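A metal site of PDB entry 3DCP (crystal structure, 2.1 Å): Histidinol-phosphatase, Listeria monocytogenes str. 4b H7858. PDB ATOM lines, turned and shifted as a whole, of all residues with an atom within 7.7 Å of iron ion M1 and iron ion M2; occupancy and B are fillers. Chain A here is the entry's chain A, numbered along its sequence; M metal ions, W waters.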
ATOM      1  N   HIS A   6     -18.429  -5.388 -29.562  1.00  0.00           N
ATOM      2  CA  HIS A   6     -17.830  -6.363 -28.665  1.00  0.00           C
ATOM      3  C   HIS A   6     -16.819  -7.260 -29.369  1.00  0.00           C
ATOM      4  O   HIS A   6     -17.191  -8.271 -29.969  1.00  0.00           O
ATOM      5  CB  HIS A   6     -18.958  -7.184 -28.022  1.00  0.00           C
ATOM      6  CG  HIS A   6     -18.553  -7.947 -26.799  1.00  0.00           C
ATOM      7  ND1 HIS A   6     -19.472  -8.361 -25.853  1.00  0.00           N
ATOM      8  CD2 HIS A   6     -17.344  -8.391 -26.373  1.00  0.00           C
ATOM      9  CE1 HIS A   6     -18.837  -9.023 -24.898  1.00  0.00           C
ATOM     10  NE2 HIS A   6     -17.554  -9.052 -25.192  1.00  0.00           N
ATOM     11  N   THR A   7     -15.550  -6.875 -29.318  1.00  0.00           N
ATOM     12  CA  THR A   7     -14.492  -7.677 -29.949  1.00  0.00           C
ATOM     13  C   THR A   7     -13.265  -7.777 -29.056  1.00  0.00           C
ATOM     14  O   THR A   7     -13.044  -6.944 -28.171  1.00  0.00           O
ATOM     15  CB  THR A   7     -14.063  -7.105 -31.305  1.00  0.00           C
ATOM     16  OG1 THR A   7     -13.326  -5.896 -31.085  1.00  0.00           O
ATOM     17  CG2 THR A   7     -15.294  -6.824 -32.180  1.00  0.00           C
ATOM     18  N   HIS A   8     -12.443  -8.794 -29.296  1.00  0.00           N
ATOM     19  CA  HIS A   8     -11.249  -9.008 -28.507  1.00  0.00           C
ATOM     20  C   HIS A   8      -9.970  -9.012 -29.348  1.00  0.00           C
ATOM     21  O   HIS A   8     -10.036  -8.887 -30.573  1.00  0.00           O
ATOM     22  CB  HIS A   8     -11.412 -10.292 -27.703  1.00  0.00           C
ATOM     23  CG  HIS A   8     -12.437 -10.183 -26.629  1.00  0.00           C
ATOM     24  ND1 HIS A   8     -12.174  -9.633 -25.390  1.00  0.00           N
ATOM     25  CD2 HIS A   8     -13.766 -10.472 -26.628  1.00  0.00           C
ATOM     26  CE1 HIS A   8     -13.276  -9.606 -24.670  1.00  0.00           C
ATOM     27  NE2 HIS A   8     -14.261 -10.105 -25.398  1.00  0.00           N
ATOM     28  N   CYS A  12      -5.786 -11.156 -25.307  1.00  0.00           N
ATOM     29  CA  CYS A  12      -6.670 -12.060 -24.579  1.00  0.00           C
ATOM     30  C   CYS A  12      -6.003 -13.419 -24.469  1.00  0.00           C
ATOM     31  O   CYS A  12      -5.777 -14.093 -25.470  1.00  0.00           O
ATOM     32  CB  CYS A  12      -8.013 -12.197 -25.307  1.00  0.00           C
ATOM     33  SG  CYS A  12      -9.133 -13.356 -24.495  1.00  0.00           S
ATOM     34  N   HIS A  14      -7.059 -16.332 -23.623  1.00  0.00           N
ATOM     35  CA  HIS A  14      -7.798 -17.467 -24.153  1.00  0.00           C
ATOM     36  C   HIS A  14      -8.314 -17.251 -25.568  1.00  0.00           C
ATOM     37  O   HIS A  14      -9.135 -18.029 -26.067  1.00  0.00           O
ATOM     38  CB  HIS A  14      -8.978 -17.818 -23.249  1.00  0.00           C
ATOM     39  CG  HIS A  14      -9.865 -16.650 -22.933  1.00  0.00           C
ATOM     40  ND1 HIS A  14      -9.580 -15.768 -21.914  1.00  0.00           N
ATOM     41  CD2 HIS A  14     -11.003 -16.206 -23.512  1.00  0.00           C
ATOM     42  CE1 HIS A  14     -10.505 -14.825 -21.888  1.00  0.00           C
ATOM     43  NE2 HIS A  14     -11.380 -15.065 -22.847  1.00  0.00           N
ATOM     44  N   VAL A  38     -13.002  -4.110 -26.867  1.00  0.00           N
ATOM     45  CA  VAL A  38     -13.258  -4.129 -25.447  1.00  0.00           C
ATOM     46  C   VAL A  38     -12.622  -5.380 -24.845  1.00  0.00           C
ATOM     47  O   VAL A  38     -13.292  -6.359 -24.528  1.00  0.00           O
ATOM     48  CB  VAL A  38     -14.762  -4.105 -25.167  1.00  0.00           C
ATOM     49  CG1 VAL A  38     -15.312  -2.708 -25.457  1.00  0.00           C
ATOM     50  CG2 VAL A  38     -15.475  -5.120 -26.071  1.00  0.00           C
ATOM     51  N   GLU A  39     -11.301  -5.337 -24.717  1.00  0.00           N
ATOM     52  CA  GLU A  39     -10.568  -6.455 -24.186  1.00  0.00           C
ATOM     53  C   GLU A  39     -10.877  -6.657 -22.693  1.00  0.00           C
ATOM     54  O   GLU A  39     -11.286  -5.733 -22.002  1.00  0.00           O
ATOM     55  CB  GLU A  39      -9.072  -6.245 -24.378  1.00  0.00           C
ATOM     56  CG  GLU A  39      -8.277  -7.462 -24.048  1.00  0.00           C
ATOM     57  CD  GLU A  39      -8.788  -8.667 -24.815  1.00  0.00           C
ATOM     58  OE1 GLU A  39      -8.460  -8.785 -26.019  1.00  0.00           O
ATOM     59  OE2 GLU A  39      -9.526  -9.462 -24.228  1.00  0.00           O
ATOM     60  N   HIS A  40     -10.685  -7.891 -22.224  1.00  0.00           N
ATOM     61  CA  HIS A  40     -10.924  -8.197 -20.824  1.00  0.00           C
ATOM     62  C   HIS A  40     -10.023  -7.405 -19.878  1.00  0.00           C
ATOM     63  O   HIS A  40      -8.791  -7.426 -20.008  1.00  0.00           O
ATOM     64  CB  HIS A  40     -10.702  -9.681 -20.568  1.00  0.00           C
ATOM     65  CG  HIS A  40     -11.744 -10.552 -21.181  1.00  0.00           C
ATOM     66  ND1 HIS A  40     -13.018 -10.664 -20.657  1.00  0.00           N
ATOM     67  CD2 HIS A  40     -11.722 -11.350 -22.270  1.00  0.00           C
ATOM     68  CE1 HIS A  40     -13.734 -11.486 -21.396  1.00  0.00           C
ATOM     69  NE2 HIS A  40     -12.970 -11.918 -22.393  1.00  0.00           N
ATOM     70  N   GLU A  93     -13.999  -4.992 -21.565  1.00  0.00           N
ATOM     71  CA  GLU A  93     -15.160  -5.776 -21.180  1.00  0.00           C
ATOM     72  C   GLU A  93     -14.831  -5.895 -19.689  1.00  0.00           C
ATOM     73  O   GLU A  93     -13.942  -6.647 -19.303  1.00  0.00           O
ATOM     74  CB  GLU A  93     -15.187  -7.160 -21.796  1.00  0.00           C
ATOM     75  CG  GLU A  93     -16.222  -8.039 -21.122  1.00  0.00           C
ATOM     76  CD  GLU A  93     -16.566  -9.275 -21.911  1.00  0.00           C
ATOM     77  OE1 GLU A  93     -15.701  -9.769 -22.642  1.00  0.00           O
ATOM     78  OE2 GLU A  93     -17.709  -9.761 -21.777  1.00  0.00           O
ATOM     79  N   VAL A  94     -15.505  -5.098 -18.869  1.00  0.00           N
ATOM     80  CA  VAL A  94     -15.234  -5.101 -17.442  1.00  0.00           C
ATOM     81  C   VAL A  94     -16.017  -6.147 -16.684  1.00  0.00           C
ATOM     82  O   VAL A  94     -17.238  -6.219 -16.785  1.00  0.00           O
ATOM     83  CB  VAL A  94     -15.533  -3.718 -16.841  1.00  0.00           C
ATOM     84  CG1 VAL A  94     -15.214  -3.721 -15.349  1.00  0.00           C
ATOM     85  CG2 VAL A  94     -14.724  -2.641 -17.570  1.00  0.00           C
ATOM     86  N   ASP A  95     -15.293  -6.967 -15.930  1.00  0.00           N
ATOM     87  CA  ASP A  95     -15.900  -8.012 -15.109  1.00  0.00           C
ATOM     88  C   ASP A  95     -16.576  -7.408 -13.892  1.00  0.00           C
ATOM     89  O   ASP A  95     -15.943  -6.649 -13.140  1.00  0.00           O
ATOM     90  CB  ASP A  95     -14.837  -8.993 -14.616  1.00  0.00           C
ATOM     91  CG  ASP A  95     -14.690 -10.200 -15.494  1.00  0.00           C
ATOM     92  OD1 ASP A  95     -15.525 -11.125 -15.386  1.00  0.00           O
ATOM     93  OD2 ASP A  95     -13.726 -10.220 -16.298  1.00  0.00           O
ATOM     94  N   VAL A 119     -18.139  -2.495 -21.897  1.00  0.00           N
ATOM     95  CA  VAL A 119     -19.173  -3.478 -21.597  1.00  0.00           C
ATOM     96  C   VAL A 119     -18.915  -3.979 -20.189  1.00  0.00           C
ATOM     97  O   VAL A 119     -17.759  -4.188 -19.801  1.00  0.00           O
ATOM     98  CB  VAL A 119     -19.100  -4.684 -22.572  1.00  0.00           C
ATOM     99  CG1 VAL A 119     -20.166  -5.712 -22.218  1.00  0.00           C
ATOM    100  CG2 VAL A 119     -19.271  -4.218 -24.016  1.00  0.00           C
ATOM    101  N   LEU A 120     -19.984  -4.137 -19.410  1.00  0.00           N
ATOM    102  CA  LEU A 120     -19.880  -4.641 -18.043  1.00  0.00           C
ATOM    103  C   LEU A 120     -20.491  -6.038 -18.096  1.00  0.00           C
ATOM    104  O   LEU A 120     -21.670  -6.188 -18.423  1.00  0.00           O
ATOM    105  CB  LEU A 120     -20.682  -3.772 -17.088  1.00  0.00           C
ATOM    106  CG  LEU A 120     -20.191  -3.542 -15.653  1.00  0.00           C
ATOM    107  CD1 LEU A 120     -21.408  -3.294 -14.753  1.00  0.00           C
ATOM    108  CD2 LEU A 120     -19.385  -4.723 -15.148  1.00  0.00           C
ATOM    109  N   SER A 121     -19.706  -7.056 -17.768  1.00  0.00           N
ATOM    110  CA  SER A 121     -20.181  -8.435 -17.840  1.00  0.00           C
ATOM    111  C   SER A 121     -20.034  -9.267 -16.575  1.00  0.00           C
ATOM    112  O   SER A 121     -19.073  -9.099 -15.808  1.00  0.00           O
ATOM    113  CB  SER A 121     -19.461  -9.172 -18.984  1.00  0.00           C
ATOM    114  OG  SER A 121     -19.653  -8.536 -20.240  1.00  0.00           O
ATOM    115  N   LEU A 122     -20.958 -10.186 -16.371  1.00  0.00           N
ATOM    116  CA  LEU A 122     -20.918 -11.076 -15.227  1.00  0.00           C
ATOM    117  C   LEU A 122     -20.369 -12.418 -15.739  1.00  0.00           C
ATOM    118  O   LEU A 122     -21.004 -13.058 -16.586  1.00  0.00           O
ATOM    119  CB  LEU A 122     -22.322 -11.256 -14.664  1.00  0.00           C
ATOM    120  CG  LEU A 122     -22.515 -11.546 -13.164  1.00  0.00           C
ATOM    121  CD1 LEU A 122     -23.647 -12.549 -12.992  1.00  0.00           C
ATOM    122  CD2 LEU A 122     -21.219 -12.063 -12.555  1.00  0.00           C
ATOM    123  N   HIS A 123     -19.210 -12.845 -15.218  1.00  0.00           N
ATOM    124  CA  HIS A 123     -18.580 -14.105 -15.629  1.00  0.00           C
ATOM    125  C   HIS A 123     -18.341 -15.069 -14.466  1.00  0.00           C
ATOM    126  O   HIS A 123     -18.140 -16.271 -14.677  1.00  0.00           O
ATOM    127  CB  HIS A 123     -17.220 -13.850 -16.297  1.00  0.00           C
ATOM    128  CG  HIS A 123     -17.306 -13.109 -17.593  1.00  0.00           C
ATOM    129  ND1 HIS A 123     -16.593 -11.949 -17.826  1.00  0.00           N
ATOM    130  CD2 HIS A 123     -18.023 -13.350 -18.719  1.00  0.00           C
ATOM    131  CE1 HIS A 123     -16.855 -11.520 -19.047  1.00  0.00           C
ATOM    132  NE2 HIS A 123     -17.726 -12.350 -19.608  1.00  0.00           N
ATOM    133  N   ASP A 135     -18.842 -19.441 -17.603  1.00  0.00           N
ATOM    134  CA  ASP A 135     -18.646 -19.840 -18.997  1.00  0.00           C
ATOM    135  C   ASP A 135     -17.410 -20.658 -19.417  1.00  0.00           C
ATOM    136  O   ASP A 135     -17.158 -20.809 -20.612  1.00  0.00           O
ATOM    137  CB  ASP A 135     -18.699 -18.569 -19.864  1.00  0.00           C
ATOM    138  CG  ASP A 135     -17.612 -17.582 -19.497  1.00  0.00           C
ATOM    139  OD1 ASP A 135     -16.916 -17.825 -18.500  1.00  0.00           O
ATOM    140  OD2 ASP A 135     -17.444 -16.563 -20.201  1.00  0.00           O
ATOM    141  N   GLY A 180     -23.131  -6.735 -20.795  1.00  0.00           N
ATOM    142  CA  GLY A 180     -22.745  -7.864 -21.626  1.00  0.00           C
ATOM    143  C   GLY A 180     -23.600  -9.132 -21.550  1.00  0.00           C
ATOM    144  O   GLY A 180     -24.038  -9.519 -20.471  1.00  0.00           O
ATOM    145  N   HIS A 181     -23.823  -9.751 -22.716  1.00  0.00           N
ATOM    146  CA  HIS A 181     -24.562 -11.017 -22.841  1.00  0.00           C
ATOM    147  C   HIS A 181     -25.342 -11.411 -21.585  1.00  0.00           C
ATOM    148  O   HIS A 181     -24.931 -12.309 -20.862  1.00  0.00           O
ATOM    149  CB  HIS A 181     -23.562 -12.130 -23.176  1.00  0.00           C
ATOM    150  CG  HIS A 181     -22.313 -12.091 -22.347  1.00  0.00           C
ATOM    151  ND1 HIS A 181     -22.323 -12.079 -20.971  1.00  0.00           N
ATOM    152  CD2 HIS A 181     -21.009 -12.043 -22.713  1.00  0.00           C
ATOM    153  CE1 HIS A 181     -21.084 -12.036 -20.512  1.00  0.00           C
ATOM    154  NE2 HIS A 181     -20.265 -12.009 -21.547  1.00  0.00           N
ATOM    155  N   LEU A 184     -25.947 -15.377 -20.202  1.00  0.00           N
ATOM    156  CA  LEU A 184     -24.771 -16.224 -20.257  1.00  0.00           C
ATOM    157  C   LEU A 184     -24.982 -17.554 -19.539  1.00  0.00           C
ATOM    158  O   LEU A 184     -24.264 -18.526 -19.782  1.00  0.00           O
ATOM    159  CB  LEU A 184     -23.571 -15.505 -19.655  1.00  0.00           C
ATOM    160  CG  LEU A 184     -22.217 -16.203 -19.882  1.00  0.00           C
ATOM    161  CD1 LEU A 184     -21.867 -16.166 -21.379  1.00  0.00           C
ATOM    162  CD2 LEU A 184     -21.155 -15.500 -19.067  1.00  0.00           C
ATOM    163  N   ASP A 222     -25.903  -5.573 -24.810  1.00  0.00           N
ATOM    164  CA  ASP A 222     -24.989  -6.236 -25.744  1.00  0.00           C
ATOM    165  C   ASP A 222     -25.773  -7.381 -26.397  1.00  0.00           C
ATOM    166  O   ASP A 222     -26.162  -8.322 -25.711  1.00  0.00           O
ATOM    167  CB  ASP A 222     -23.799  -6.754 -24.916  1.00  0.00           C
ATOM    168  CG  ASP A 222     -22.878  -7.701 -25.671  1.00  0.00           C
ATOM    169  OD1 ASP A 222     -22.495  -7.407 -26.819  1.00  0.00           O
ATOM    170  OD2 ASP A 222     -22.481  -8.732 -25.072  1.00  0.00           O
ATOM    171  N   ASN A 224     -25.336 -10.176 -28.126  1.00  0.00           N
ATOM    172  CA  ASN A 224     -24.214 -11.063 -28.366  1.00  0.00           C
ATOM    173  C   ASN A 224     -24.559 -12.346 -29.130  1.00  0.00           C
ATOM    174  O   ASN A 224     -25.352 -13.171 -28.672  1.00  0.00           O
ATOM    175  CB  ASN A 224     -23.604 -11.391 -26.998  1.00  0.00           C
ATOM    176  CG  ASN A 224     -22.194 -11.914 -27.091  1.00  0.00           C
ATOM    177  OD1 ASN A 224     -21.934 -12.907 -27.778  1.00  0.00           O
ATOM    178  ND2 ASN A 224     -21.275 -11.268 -26.378  1.00  0.00           N
ATOM    179  N   ALA A 226     -22.313 -14.684 -30.000  1.00  0.00           N
ATOM    180  CA  ALA A 226     -21.348 -15.739 -29.712  1.00  0.00           C
ATOM    181  C   ALA A 226     -22.057 -17.066 -29.418  1.00  0.00           C
ATOM    182  O   ALA A 226     -21.583 -18.123 -29.820  1.00  0.00           O
ATOM    183  CB  ALA A 226     -20.475 -15.346 -28.518  1.00  0.00           C
ATOM    184  N   SER A 257     -20.264  -9.349 -31.672  1.00  0.00           N
ATOM    185  CA  SER A 257     -19.811 -10.631 -32.202  1.00  0.00           C
ATOM    186  C   SER A 257     -18.963 -11.371 -31.177  1.00  0.00           C
ATOM    187  O   SER A 257     -18.767 -12.586 -31.282  1.00  0.00           O
ATOM    188  CB  SER A 257     -18.959 -10.406 -33.446  1.00  0.00           C
ATOM    189  OG  SER A 257     -17.706  -9.834 -33.096  1.00  0.00           O
ATOM    190  N   ASP A 258     -18.452 -10.640 -30.197  1.00  0.00           N
ATOM    191  CA  ASP A 258     -17.600 -11.225 -29.169  1.00  0.00           C
ATOM    192  C   ASP A 258     -16.456 -11.984 -29.861  1.00  0.00           C
ATOM    193  O   ASP A 258     -16.038 -13.051 -29.398  1.00  0.00           O
ATOM    194  CB  ASP A 258     -18.406 -12.196 -28.299  1.00  0.00           C
ATOM    195  CG  ASP A 258     -17.947 -12.165 -26.851  1.00  0.00           C
ATOM    196  OD1 ASP A 258     -16.766 -11.883 -26.598  1.00  0.00           O
ATOM    197  OD2 ASP A 258     -18.780 -12.442 -25.958  1.00  0.00           O
ATOM    198  N   SER A 259     -15.947 -11.428 -30.951  1.00  0.00           N
ATOM    199  CA  SER A 259     -14.876 -12.058 -31.722  1.00  0.00           C
ATOM    200  C   SER A 259     -13.554 -12.173 -30.972  1.00  0.00           C
ATOM    201  O   SER A 259     -13.087 -11.209 -30.342  1.00  0.00           O
ATOM    202  CB  SER A 259     -14.637 -11.301 -33.037  1.00  0.00           C
ATOM    203  OG  SER A 259     -15.759 -11.365 -33.902  1.00  0.00           O
ATOM    204  N   HIS A 260     -12.945 -13.350 -31.032  1.00  0.00           N
ATOM    205  CA  HIS A 260     -11.652 -13.603 -30.409  1.00  0.00           C
ATOM    206  C   HIS A 260     -10.664 -14.016 -31.485  1.00  0.00           C
ATOM    207  O   HIS A 260      -9.568 -14.499 -31.202  1.00  0.00           O
ATOM    208  CB  HIS A 260     -11.757 -14.715 -29.359  1.00  0.00           C
ATOM    209  CG  HIS A 260     -12.550 -14.324 -28.149  1.00  0.00           C
ATOM    210  ND1 HIS A 260     -13.908 -14.078 -28.211  1.00  0.00           N
ATOM    211  CD2 HIS A 260     -12.179 -14.085 -26.878  1.00  0.00           C
ATOM    212  CE1 HIS A 260     -14.339 -13.709 -27.017  1.00  0.00           C
ATOM    213  NE2 HIS A 260     -13.314 -13.702 -26.188  1.00  0.00           N
HETATM  214 FE    FE M   1     -16.262 -10.763 -24.590  1.00  0.00          FE
HETATM  215 FE    FE M   2     -17.948 -12.038 -21.737  1.00  0.00          FE
HETATM  216 ZN    ZN M   3     -12.897 -13.656 -23.952  1.00  0.00          ZN
HETATM  217  O   HOH W   1     -18.721 -14.350 -21.836  1.00  0.00           O
HETATM  218  O   HOH W   2     -15.683 -13.867 -23.529  1.00  0.00           O
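OD1 of Asp 95 sits at hydrogen-bond distance from ND1 of His 123 (2.8 Å).
ND1 of His 6 lies within hydrogen-bond range of OD2 of Asp 222 (3.1 Å).
The backbone NH (N) of His 8 is in hydrogen-bond range of the backbone carbonyl oxygen (O) of Ser 259.
The side-chain carboxylate (OE2) of Glu 39 is in hydrogen-bond range of a ring nitrogen (ND1) of His 8.
A ring nitrogen (ND1) of His 40 lies close to the side-chain carboxylate (OE1) of Glu 93, 3.5 Å away.
The backbone NH (N) of Glu 93 sits at hydrogen-bond distance from the backbone carbonyl oxygen (O) of Val 38 (3.3 Å).
OD2 of Asp 222 is in hydrogen-bond range of N of His 181 (2.9 Å).
OD2 of Asp 258 lies within hydrogen-bond range of ND2 of Asn 224, at 2.8 Å.
Three residues have an atom within 4 Å of iron ion M2: Glu 93, His 123 and His 181.
The nearest printed residue that does not touch iron ion M2 is Ser 121 (4.2 Å).
Iron ion M1 is bound by NE2 of His 6, NE2 of His 8, OE1 of Glu 93 and OD1 of Asp 258.
NE2 of His 123 binds iron ion M2.
Iron ion M2 is bound by OE2 of Glu 93 (2.3 Å).
NE2 of His 181 is bound to iron ion M2, 2.3 Å away.
Iron ion M2 is bound by water W1, 2.4 Å away.
Iron ion M2 has four donor atoms within binding distance.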
